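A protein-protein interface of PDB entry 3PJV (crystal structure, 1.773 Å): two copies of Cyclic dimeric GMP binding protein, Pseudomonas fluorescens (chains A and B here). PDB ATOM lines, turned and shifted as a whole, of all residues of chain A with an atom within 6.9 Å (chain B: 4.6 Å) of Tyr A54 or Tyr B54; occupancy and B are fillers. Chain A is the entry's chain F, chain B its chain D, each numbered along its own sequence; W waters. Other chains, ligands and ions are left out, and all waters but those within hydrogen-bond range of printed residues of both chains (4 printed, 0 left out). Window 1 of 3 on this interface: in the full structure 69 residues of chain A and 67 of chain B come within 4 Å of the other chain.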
ATOM      1  N   GLN A  16      29.644  14.202 -16.528  1.00  0.00           N
ATOM      2  CA  GLN A  16      28.800  15.145 -15.807  1.00  0.00           C
ATOM      3  C   GLN A  16      27.341  14.702 -15.843  1.00  0.00           C
ATOM      4  O   GLN A  16      26.653  14.749 -14.828  1.00  0.00           O
ATOM      5  CB  GLN A  16      28.956  16.564 -16.363  1.00  0.00           C
ATOM      6  CG  GLN A  16      28.194  17.624 -15.566  1.00  0.00           C
ATOM      7  CD  GLN A  16      26.726  17.717 -15.959  1.00  0.00           C
ATOM      8  OE1 GLN A  16      25.857  18.018 -15.132  1.00  0.00           O
ATOM      9  NE2 GLN A  16      26.445  17.458 -17.231  1.00  0.00           N
ATOM     10  N   LEU A  17      26.877  14.261 -17.013  1.00  0.00           N
ATOM     11  CA  LEU A  17      25.513  13.780 -17.148  1.00  0.00           C
ATOM     12  C   LEU A  17      25.283  12.563 -16.259  1.00  0.00           C
ATOM     13  O   LEU A  17      24.238  12.441 -15.625  1.00  0.00           O
ATOM     14  CB  LEU A  17      25.190  13.442 -18.608  1.00  0.00           C
ATOM     15  CG  LEU A  17      25.136  14.628 -19.577  1.00  0.00           C
ATOM     16  CD1 LEU A  17      24.947  14.104 -20.992  1.00  0.00           C
ATOM     17  CD2 LEU A  17      24.020  15.585 -19.197  1.00  0.00           C
ATOM     18  N   HIS A  20      25.278  13.639 -12.476  1.00  0.00           N
ATOM     19  CA  HIS A  20      24.052  14.397 -12.242  1.00  0.00           C
ATOM     20  C   HIS A  20      22.867  13.437 -12.111  1.00  0.00           C
ATOM     21  O   HIS A  20      22.046  13.568 -11.206  1.00  0.00           O
ATOM     22  CB  HIS A  20      23.834  15.387 -13.394  1.00  0.00           C
ATOM     23  CG  HIS A  20      22.592  16.216 -13.268  1.00  0.00           C
ATOM     24  ND1 HIS A  20      21.467  15.987 -14.034  1.00  0.00           N
ATOM     25  CD2 HIS A  20      22.302  17.282 -12.485  1.00  0.00           C
ATOM     26  CE1 HIS A  20      20.537  16.873 -13.721  1.00  0.00           C
ATOM     27  NE2 HIS A  20      21.016  17.668 -12.781  1.00  0.00           N
ATOM     28  N   ILE A  49      10.682  16.008  -8.472  1.00  0.00           N
ATOM     29  CA  ILE A  49      12.081  16.052  -8.885  1.00  0.00           C
ATOM     30  C   ILE A  49      12.175  16.316 -10.380  1.00  0.00           C
ATOM     31  O   ILE A  49      12.954  17.156 -10.834  1.00  0.00           O
ATOM     32  CB  ILE A  49      12.816  14.740  -8.546  1.00  0.00           C
ATOM     33  CG1 ILE A  49      12.904  14.575  -7.025  1.00  0.00           C
ATOM     34  CG2 ILE A  49      14.216  14.731  -9.151  1.00  0.00           C
ATOM     35  CD1 ILE A  49      13.643  15.713  -6.340  1.00  0.00           C
ATOM     36  N   PHE A  50      11.362  15.599 -11.144  1.00  0.00           N
ATOM     37  CA  PHE A  50      11.365  15.762 -12.591  1.00  0.00           C
ATOM     38  C   PHE A  50      11.061  17.197 -12.996  1.00  0.00           C
ATOM     39  O   PHE A  50      11.697  17.750 -13.889  1.00  0.00           O
ATOM     40  CB  PHE A  50      10.374  14.804 -13.263  1.00  0.00           C
ATOM     41  CG  PHE A  50      10.504  14.778 -14.764  1.00  0.00           C
ATOM     42  CD1 PHE A  50       9.679  15.553 -15.564  1.00  0.00           C
ATOM     43  CD2 PHE A  50      11.486  14.014 -15.361  1.00  0.00           C
ATOM     44  CE1 PHE A  50       9.821  15.544 -16.943  1.00  0.00           C
ATOM     45  CE2 PHE A  50      11.635  14.000 -16.748  1.00  0.00           C
ATOM     46  CZ  PHE A  50      10.803  14.771 -17.529  1.00  0.00           C
ATOM     47  N   ASP A  51      10.087  17.803 -12.329  1.00  0.00           N
ATOM     48  CA  ASP A  51       9.638  19.141 -12.703  1.00  0.00           C
ATOM     49  C   ASP A  51      10.603  20.266 -12.311  1.00  0.00           C
ATOM     50  O   ASP A  51      10.536  21.356 -12.866  1.00  0.00           O
ATOM     51  CB  ASP A  51       8.241  19.418 -12.132  1.00  0.00           C
ATOM     52  CG  ASP A  51       7.161  18.573 -12.793  1.00  0.00           C
ATOM     53  OD1 ASP A  51       7.373  18.122 -13.937  1.00  0.00           O
ATOM     54  OD2 ASP A  51       6.099  18.365 -12.168  1.00  0.00           O
ATOM     55  N   SER A  52      11.491  20.011 -11.358  1.00  0.00           N
ATOM     56  CA  SER A  52      12.407  21.059 -10.897  1.00  0.00           C
ATOM     57  C   SER A  52      13.838  20.869 -11.395  1.00  0.00           C
ATOM     58  O   SER A  52      14.744  21.591 -10.987  1.00  0.00           O
ATOM     59  CB  SER A  52      12.389  21.153  -9.368  1.00  0.00           C
ATOM     60  OG  SER A  52      12.788  19.929  -8.778  1.00  0.00           O
ATOM     61  N   GLY A  53      14.035  19.895 -12.278  1.00  0.00           N
ATOM     62  CA  GLY A  53      15.357  19.583 -12.790  1.00  0.00           C
ATOM     63  C   GLY A  53      15.395  19.434 -14.303  1.00  0.00           C
ATOM     64  O   GLY A  53      14.388  19.625 -14.985  1.00  0.00           O
ATOM     65  N   TYR A  54      16.571  19.098 -14.821  1.00  0.00           N
ATOM     66  CA  TYR A  54      16.797  18.998 -16.267  1.00  0.00           C
ATOM     67  C   TYR A  54      17.030  17.549 -16.660  1.00  0.00           C
ATOM     68  O   TYR A  54      18.171  17.127 -16.839  1.00  0.00           O
ATOM     69  CB  TYR A  54      18.018  19.827 -16.661  1.00  0.00           C
ATOM     70  CG  TYR A  54      17.868  21.320 -16.412  1.00  0.00           C
ATOM     71  CD1 TYR A  54      16.610  21.930 -16.387  1.00  0.00           C
ATOM     72  CD2 TYR A  54      18.986  22.122 -16.237  1.00  0.00           C
ATOM     73  CE1 TYR A  54      16.483  23.296 -16.175  1.00  0.00           C
ATOM     74  CE2 TYR A  54      18.870  23.477 -16.037  1.00  0.00           C
ATOM     75  CZ  TYR A  54      17.619  24.064 -15.999  1.00  0.00           C
ATOM     76  OH  TYR A  54      17.518  25.422 -15.808  1.00  0.00           O
ATOM     77  N   TYR A  55      15.943  16.790 -16.787  1.00  0.00           N
ATOM     78  CA  TYR A  55      16.024  15.345 -16.999  1.00  0.00           C
ATOM     79  C   TYR A  55      15.329  14.916 -18.293  1.00  0.00           C
ATOM     80  O   TYR A  55      14.293  15.464 -18.648  1.00  0.00           O
ATOM     81  CB  TYR A  55      15.394  14.597 -15.818  1.00  0.00           C
ATOM     82  CG  TYR A  55      16.031  14.937 -14.482  1.00  0.00           C
ATOM     83  CD1 TYR A  55      17.294  14.452 -14.152  1.00  0.00           C
ATOM     84  CD2 TYR A  55      15.375  15.762 -13.566  1.00  0.00           C
ATOM     85  CE1 TYR A  55      17.887  14.776 -12.941  1.00  0.00           C
ATOM     86  CE2 TYR A  55      15.962  16.079 -12.349  1.00  0.00           C
ATOM     87  CZ  TYR A  55      17.219  15.590 -12.050  1.00  0.00           C
ATOM     88  OH  TYR A  55      17.811  15.910 -10.849  1.00  0.00           O
ATOM     89  N   SER A  56      15.910  13.943 -18.989  1.00  0.00           N
ATOM     90  CA  SER A  56      15.246  13.312 -20.126  1.00  0.00           C
ATOM     91  C   SER A  56      14.144  12.371 -19.661  1.00  0.00           C
ATOM     92  O   SER A  56      13.076  12.281 -20.273  1.00  0.00           O
ATOM     93  CB  SER A  56      16.243  12.513 -20.979  1.00  0.00           C
ATOM     94  OG  SER A  56      17.080  13.374 -21.726  1.00  0.00           O
ATOM     95  N   SER A  57      14.421  11.639 -18.591  1.00  0.00           N
ATOM     96  CA  SER A  57      13.443  10.708 -18.067  1.00  0.00           C
ATOM     97  C   SER A  57      13.752  10.334 -16.629  1.00  0.00           C
ATOM     98  O   SER A  57      14.903  10.367 -16.201  1.00  0.00           O
ATOM     99  CB  SER A  57      13.408   9.435 -18.914  1.00  0.00           C
ATOM    100  OG  SER A  57      14.680   8.804 -18.936  1.00  0.00           O
ATOM    101  N   VAL A 112      25.531  34.320  -9.836  1.00  0.00           N
ATOM    102  CA  VAL A 112      25.196  33.266 -10.795  1.00  0.00           C
ATOM    103  C   VAL A 112      24.102  33.761 -11.720  1.00  0.00           C
ATOM    104  O   VAL A 112      23.198  34.456 -11.284  1.00  0.00           O
ATOM    105  CB  VAL A 112      24.709  31.976 -10.075  1.00  0.00           C
ATOM    106  CG1 VAL A 112      24.211  30.933 -11.098  1.00  0.00           C
ATOM    107  CG2 VAL A 112      25.822  31.403  -9.198  1.00  0.00           C
ATOM    108  N   VAL A 113      24.201  33.427 -13.004  1.00  0.00           N
ATOM    109  CA  VAL A 113      23.098  33.652 -13.927  1.00  0.00           C
ATOM    110  C   VAL A 113      22.771  32.322 -14.582  1.00  0.00           C
ATOM    111  O   VAL A 113      23.662  31.677 -15.171  1.00  0.00           O
ATOM    112  CB  VAL A 113      23.466  34.667 -15.026  1.00  0.00           C
ATOM    113  CG1 VAL A 113      22.315  34.809 -16.014  1.00  0.00           C
ATOM    114  CG2 VAL A 113      23.757  36.022 -14.410  1.00  0.00           C
ATOM    115  N   SER A 114      21.511  31.898 -14.485  1.00  0.00           N
ATOM    116  CA  SER A 114      21.123  30.582 -15.012  1.00  0.00           C
ATOM    117  C   SER A 114      20.696  30.681 -16.473  1.00  0.00           C
ATOM    118  O   SER A 114      19.970  31.598 -16.850  1.00  0.00           O
ATOM    119  CB  SER A 114      19.992  29.970 -14.175  1.00  0.00           C
ATOM    120  OG  SER A 114      20.475  29.582 -12.900  1.00  0.00           O
ATOM    121  N   HIS A 115      21.149  29.732 -17.292  1.00  0.00           N
ATOM    122  CA  HIS A 115      20.827  29.782 -18.716  1.00  0.00           C
ATOM    123  C   HIS A 115      19.368  29.395 -18.948  1.00  0.00           C
ATOM    124  O   HIS A 115      18.911  28.385 -18.431  1.00  0.00           O
ATOM    125  CB  HIS A 115      21.735  28.828 -19.494  1.00  0.00           C
ATOM    126  CG  HIS A 115      21.810  29.141 -20.957  1.00  0.00           C
ATOM    127  ND1 HIS A 115      20.741  28.962 -21.811  1.00  0.00           N
ATOM    128  CD2 HIS A 115      22.820  29.635 -21.713  1.00  0.00           C
ATOM    129  CE1 HIS A 115      21.093  29.335 -23.033  1.00  0.00           C
ATOM    130  NE2 HIS A 115      22.347  29.744 -23.000  1.00  0.00           N
ATOM    131  N   PRO A 116      18.639  30.199 -19.745  1.00  0.00           N
ATOM    132  CA  PRO A 116      17.199  30.010 -19.957  1.00  0.00           C
ATOM    133  C   PRO A 116      16.836  28.990 -21.045  1.00  0.00           C
ATOM    134  O   PRO A 116      15.640  28.782 -21.292  1.00  0.00           O
ATOM    135  CB  PRO A 116      16.739  31.400 -20.391  1.00  0.00           C
ATOM    136  CG  PRO A 116      17.913  31.944 -21.146  1.00  0.00           C
ATOM    137  CD  PRO A 116      19.135  31.420 -20.410  1.00  0.00           C
ATOM    138  N   MET A 117      17.821  28.358 -21.675  1.00  0.00           N
ATOM    139  CA  MET A 117      17.491  27.503 -22.834  1.00  0.00           C
ATOM    140  C   MET A 117      16.455  26.413 -22.504  1.00  0.00           C
ATOM    141  O   MET A 117      15.532  26.177 -23.288  1.00  0.00           O
ATOM    142  CB  MET A 117      18.746  26.919 -23.507  1.00  0.00           C
ATOM    143  CG  MET A 117      19.417  25.797 -22.765  1.00  0.00           C
ATOM    144  SD  MET A 117      20.627  24.812 -24.016  1.00  0.00           S
ATOM    145  CE  MET A 117      20.053  25.631 -25.748  1.00  0.00           C
ATOM    146  N   PHE A 118      16.580  25.762 -21.347  1.00  0.00           N
ATOM    147  CA  PHE A 118      15.651  24.681 -20.968  1.00  0.00           C
ATOM    148  C   PHE A 118      14.228  25.195 -20.722  1.00  0.00           C
ATOM    149  O   PHE A 118      13.251  24.605 -21.189  1.00  0.00           O
ATOM    150  CB  PHE A 118      16.157  23.887 -19.742  1.00  0.00           C
ATOM    151  CG  PHE A 118      15.554  22.503 -19.620  1.00  0.00           C
ATOM    152  CD1 PHE A 118      14.412  22.298 -18.869  1.00  0.00           C
ATOM    153  CD2 PHE A 118      16.125  21.415 -20.267  1.00  0.00           C
ATOM    154  CE1 PHE A 118      13.849  21.036 -18.752  1.00  0.00           C
ATOM    155  CE2 PHE A 118      15.561  20.142 -20.152  1.00  0.00           C
ATOM    156  CZ  PHE A 118      14.421  19.961 -19.394  1.00  0.00           C
ATOM    157  N   ALA A 119      14.122  26.304 -19.991  1.00  0.00           N
ATOM    158  CA  ALA A 119      12.829  26.955 -19.755  1.00  0.00           C
ATOM    159  C   ALA A 119      12.132  27.322 -21.069  1.00  0.00           C
ATOM    160  O   ALA A 119      10.945  27.066 -21.247  1.00  0.00           O
ATOM    161  CB  ALA A 119      13.020  28.214 -18.890  1.00  0.00           C
ATOM    162  N   LYS A 122      10.826  24.322 -22.951  1.00  0.00           N
ATOM    163  CA  LYS A 122       9.605  23.831 -22.316  1.00  0.00           C
ATOM    164  C   LYS A 122       8.388  24.680 -22.657  1.00  0.00           C
ATOM    165  O   LYS A 122       7.316  24.150 -22.950  1.00  0.00           O
ATOM    166  CB  LYS A 122       9.774  23.764 -20.797  1.00  0.00           C
ATOM    167  CG  LYS A 122      10.438  22.489 -20.308  1.00  0.00           C
ATOM    168  CD  LYS A 122      10.487  22.431 -18.785  1.00  0.00           C
ATOM    169  CE  LYS A 122       9.142  22.021 -18.202  1.00  0.00           C
ATOM    170  NZ  LYS A 122       9.173  21.935 -16.708  1.00  0.00           N
ATOM    171  N   LEU B  17      13.601  29.807 -12.777  1.00  0.00           N
ATOM    172  CA  LEU B  17      14.987  30.078 -13.189  1.00  0.00           C
ATOM    173  C   LEU B  17      15.713  30.918 -12.153  1.00  0.00           C
ATOM    174  O   LEU B  17      16.886  30.682 -11.849  1.00  0.00           O
ATOM    175  CB  LEU B  17      15.031  30.820 -14.520  1.00  0.00           C
ATOM    176  CG  LEU B  17      14.870  30.036 -15.812  1.00  0.00           C
ATOM    177  CD1 LEU B  17      14.928  31.015 -16.978  1.00  0.00           C
ATOM    178  CD2 LEU B  17      15.969  28.983 -15.911  1.00  0.00           C
ATOM    179  N   HIS B  20      16.621  28.781  -9.407  1.00  0.00           N
ATOM    180  CA  HIS B  20      17.713  27.917  -9.846  1.00  0.00           C
ATOM    181  C   HIS B  20      19.058  28.634  -9.643  1.00  0.00           C
ATOM    182  O   HIS B  20      20.010  28.064  -9.096  1.00  0.00           O
ATOM    183  CB  HIS B  20      17.492  27.519 -11.310  1.00  0.00           C
ATOM    184  CG  HIS B  20      18.505  26.558 -11.845  1.00  0.00           C
ATOM    185  ND1 HIS B  20      19.679  26.968 -12.441  1.00  0.00           N
ATOM    186  CD2 HIS B  20      18.510  25.203 -11.897  1.00  0.00           C
ATOM    187  CE1 HIS B  20      20.360  25.908 -12.845  1.00  0.00           C
ATOM    188  NE2 HIS B  20      19.678  24.825 -12.516  1.00  0.00           N
ATOM    189  N   SER B  52      28.678  22.048 -15.884  1.00  0.00           N
ATOM    190  CA  SER B  52      27.417  21.437 -16.312  1.00  0.00           C
ATOM    191  C   SER B  52      26.857  22.121 -17.553  1.00  0.00           C
ATOM    192  O   SER B  52      26.115  21.515 -18.331  1.00  0.00           O
ATOM    193  CB  SER B  52      26.372  21.525 -15.196  1.00  0.00           C
ATOM    194  OG  SER B  52      26.095  22.879 -14.865  1.00  0.00           O
ATOM    195  N   GLY B  53      27.163  23.409 -17.700  1.00  0.00           N
ATOM    196  CA  GLY B  53      26.600  24.185 -18.789  1.00  0.00           C
ATOM    197  C   GLY B  53      25.281  24.849 -18.422  1.00  0.00           C
ATOM    198  O   GLY B  53      24.711  25.566 -19.231  1.00  0.00           O
ATOM    199  N   TYR B  54      24.800  24.621 -17.196  1.00  0.00           N
ATOM    200  CA  TYR B  54      23.486  25.142 -16.802  1.00  0.00           C
ATOM    201  C   TYR B  54      23.482  26.649 -16.548  1.00  0.00           C
ATOM    202  O   TYR B  54      22.411  27.254 -16.427  1.00  0.00           O
ATOM    203  CB  TYR B  54      22.950  24.457 -15.538  1.00  0.00           C
ATOM    204  CG  TYR B  54      22.816  22.952 -15.621  1.00  0.00           C
ATOM    205  CD1 TYR B  54      22.617  22.312 -16.835  1.00  0.00           C
ATOM    206  CD2 TYR B  54      22.893  22.171 -14.469  1.00  0.00           C
ATOM    207  CE1 TYR B  54      22.498  20.930 -16.903  1.00  0.00           C
ATOM    208  CE2 TYR B  54      22.780  20.797 -14.527  1.00  0.00           C
ATOM    209  CZ  TYR B  54      22.587  20.178 -15.740  1.00  0.00           C
ATOM    210  OH  TYR B  54      22.477  18.809 -15.789  1.00  0.00           O
ATOM    211  N   TYR B  55      24.667  27.243 -16.434  1.00  0.00           N
ATOM    212  CA  TYR B  55      24.776  28.654 -16.045  1.00  0.00           C
ATOM    213  C   TYR B  55      25.421  29.491 -17.144  1.00  0.00           C
ATOM    214  O   TYR B  55      26.446  29.092 -17.708  1.00  0.00           O
ATOM    215  CB  TYR B  55      25.537  28.797 -14.710  1.00  0.00           C
ATOM    216  CG  TYR B  55      24.951  27.875 -13.674  1.00  0.00           C
ATOM    217  CD1 TYR B  55      23.787  28.222 -12.999  1.00  0.00           C
ATOM    218  CD2 TYR B  55      25.507  26.624 -13.440  1.00  0.00           C
ATOM    219  CE1 TYR B  55      23.208  27.360 -12.088  1.00  0.00           C
ATOM    220  CE2 TYR B  55      24.941  25.759 -12.526  1.00  0.00           C
ATOM    221  CZ  TYR B  55      23.788  26.138 -11.850  1.00  0.00           C
ATOM    222  OH  TYR B  55      23.207  25.281 -10.945  1.00  0.00           O
ATOM    223  N   SER B  56      24.802  30.632 -17.467  1.00  0.00           N
ATOM    224  CA  SER B  56      25.379  31.571 -18.430  1.00  0.00           C
ATOM    225  C   SER B  56      26.668  32.182 -17.888  1.00  0.00           C
ATOM    226  O   SER B  56      27.591  32.515 -18.647  1.00  0.00           O
ATOM    227  CB  SER B  56      24.387  32.708 -18.731  1.00  0.00           C
ATOM    228  OG  SER B  56      23.168  32.203 -19.248  1.00  0.00           O
ATOM    229  N   SER B 114      19.787  12.188 -17.496  1.00  0.00           N
ATOM    230  CA  SER B 114      19.916  13.645 -17.506  1.00  0.00           C
ATOM    231  C   SER B 114      19.764  14.207 -18.910  1.00  0.00           C
ATOM    232  O   SER B 114      20.247  13.615 -19.868  1.00  0.00           O
ATOM    233  CB  SER B 114      21.272  14.060 -16.927  1.00  0.00           C
ATOM    234  OG  SER B 114      21.362  13.628 -15.584  1.00  0.00           O
ATOM    235  N   HIS B 115      19.099  15.348 -19.033  1.00  0.00           N
ATOM    236  CA  HIS B 115      18.891  15.914 -20.374  1.00  0.00           C
ATOM    237  C   HIS B 115      20.197  16.466 -20.952  1.00  0.00           C
ATOM    238  O   HIS B 115      20.890  17.243 -20.289  1.00  0.00           O
ATOM    239  CB  HIS B 115      17.808  17.002 -20.339  1.00  0.00           C
ATOM    240  CG  HIS B 115      17.168  17.247 -21.672  1.00  0.00           C
ATOM    241  ND1 HIS B 115      17.826  17.865 -22.714  1.00  0.00           N
ATOM    242  CD2 HIS B 115      15.937  16.926 -22.143  1.00  0.00           C
ATOM    243  CE1 HIS B 115      17.025  17.930 -23.762  1.00  0.00           C
ATOM    244  NE2 HIS B 115      15.872  17.367 -23.442  1.00  0.00           N
ATOM    245  N   PHE B 118      22.279  20.943 -22.825  1.00  0.00           N
ATOM    246  CA  PHE B 118      23.382  21.863 -22.577  1.00  0.00           C
ATOM    247  C   PHE B 118      24.699  21.276 -23.066  1.00  0.00           C
ATOM    248  O   PHE B 118      25.545  21.985 -23.615  1.00  0.00           O
ATOM    249  CB  PHE B 118      23.473  22.227 -21.083  1.00  0.00           C
ATOM    250  CG  PHE B 118      22.241  22.918 -20.551  1.00  0.00           C
ATOM    251  CD1 PHE B 118      22.110  24.297 -20.641  1.00  0.00           C
ATOM    252  CD2 PHE B 118      21.204  22.183 -19.997  1.00  0.00           C
ATOM    253  CE1 PHE B 118      20.973  24.933 -20.158  1.00  0.00           C
ATOM    254  CE2 PHE B 118      20.062  22.815 -19.524  1.00  0.00           C
ATOM    255  CZ  PHE B 118      19.951  24.189 -19.601  1.00  0.00           C
HETATM  256  O   HOH W   1      19.668  26.869 -16.403  1.00  0.00           O
HETATM  257  O   HOH W   2      20.932  17.881 -17.577  1.00  0.00           O
HETATM  258  O   HOH W   3      24.848  19.058 -18.871  1.00  0.00           O
HETATM  259  O   HOH W   4      22.351  10.930 -17.835  1.00  0.00           O
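Tyr A54 touches Leu B17, but with the chains exchanged Leu A17 does not touch Tyr B54 (4.9 Å).
Tyr A54 touches Ser B114, and with the chains exchanged Ser A114 touches Tyr B54.
Tyr A54 touches His B115, and with the chains exchanged His A115 touches Tyr B54.
Phe A118 touches His B115, but with the chains exchanged His A115 does not touch Phe B118 (4.02 Å).
Positions printed for both chains: 17, 20, 52, 53, 54, 55, 56, 114, 115 and 118.
Of the 31 pairs that touch across the chains among the printed residues, 18 have their exchanged pair printed and touching as well.
The backbone NH (N) of His B115 lies within hydrogen-bond range of the backbone carbonyl oxygen (O) of Tyr A54, 3.0 Å away.
O of Val A113 lies within hydrogen-bond range of N of Ser B56, at 2.8 Å.
O of Leu A17 lies within hydrogen-bond range of OG of Ser B114 (3.1 Å).
N of His B115 sits close to N of Ser A56 (3.5 Å).
The side-chain hydroxyl of Ser B114 sits at hydrogen-bond distance from a ring nitrogen (ND1) of His A20, at 2.8 Å.
The side-chain hydroxyl (OH) of Tyr B54 lies close to a ring nitrogen (ND1) of His A20, 3.5 Å away.
ND1 of His B20 is in hydrogen-bond range of OG of Ser A114 (2.8 Å).
N of His A115 sits at hydrogen-bond distance from O of Tyr B54, at 2.9 Å.
Water W2 lies within hydrogen-bond range of the side-chain hydroxyl (OH) of Tyr B54, the backbone carbonyl oxygen (O) of His B115 and the backbone carbonyl oxygen (O) of Tyr A54.
Water W1 lies within hydrogen-bond range of the backbone carbonyl oxygen of His A115 (2.6 Å), the side-chain hydroxyl of Tyr A54 (2.7 Å) and the backbone carbonyl oxygen of Tyr B54 (2.8 Å).
Water W3 bridges the side-chain amide nitrogen (NE2) of Gln A16 and the backbone carbonyl oxygen (O) of Ser B52.
Water W4 bridges the backbone NH of Ser B114 (2.9 Å) and the backbone carbonyl oxygen of Leu A17 (3.3 Å).
Of the printed residues of chain B, Gln A16 touches Ser B52 (3.5 Å) and Tyr B54 (3.5 Å).
Phe A50 touches none of the printed residues of chain B.
No residue of chain A comes within 4 Å of Gly B53.
Tyr B54 touches just these residues of chain A: Gln A16, His A20, Tyr A54, Ser A114 and His A115.
Of the printed residues of chain A, Tyr B55 touches Val A112, Val A113, Ser A114 and His A115.
The nearest residue of chain A that does not touch Tyr B54 is Val A113 (4.8 Å).
The nearest printed residue of chain B that does not touch Val A112 is His B20 (5.5 Å).
The backbone NH (N) of Tyr B54 is in hydrogen-bond range of the side-chain hydroxyl (OG) of Ser B52, 3.2 Å away.
ND1 of His A115 lies within hydrogen-bond range of N of Met A117 (3.0 Å).
Tyr B54 touches Tyr A54 (CD1 to CD2, 3.7 Å).
CE2 of Phe B118 touches CD2 of Tyr A54, at 3.5 Å.
Tyr A55 touches His B115 (CA to N, 3.7 Å).
O of Ser B114 touches OG of Ser A56, 3.7 Å away.
Tyr B55 touches Val A112 (CD1 to CG1, 3.3 Å).
O of Tyr B54 touches C of Ser A114, 3.8 Å away.
O of His A115 touches CD2 of Leu B17, at 3.9 Å.
Tyr B55 touches His A115.
Phe B118 touches Met A117 (CE1 to CG, 3.2 Å).
Phe B118 touches Phe A118 (CZ to CB, 3.8 Å).
Hydrophobic or aromatic side chains of chain A within 4 Å of the printed part of chain B: Leu A17, His A20, Tyr A54, Val A112, His A115, Pro A116, Met A117, Phe A118 and Ala A119.
Among the printed residues, 31 pairs touch across the chains.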
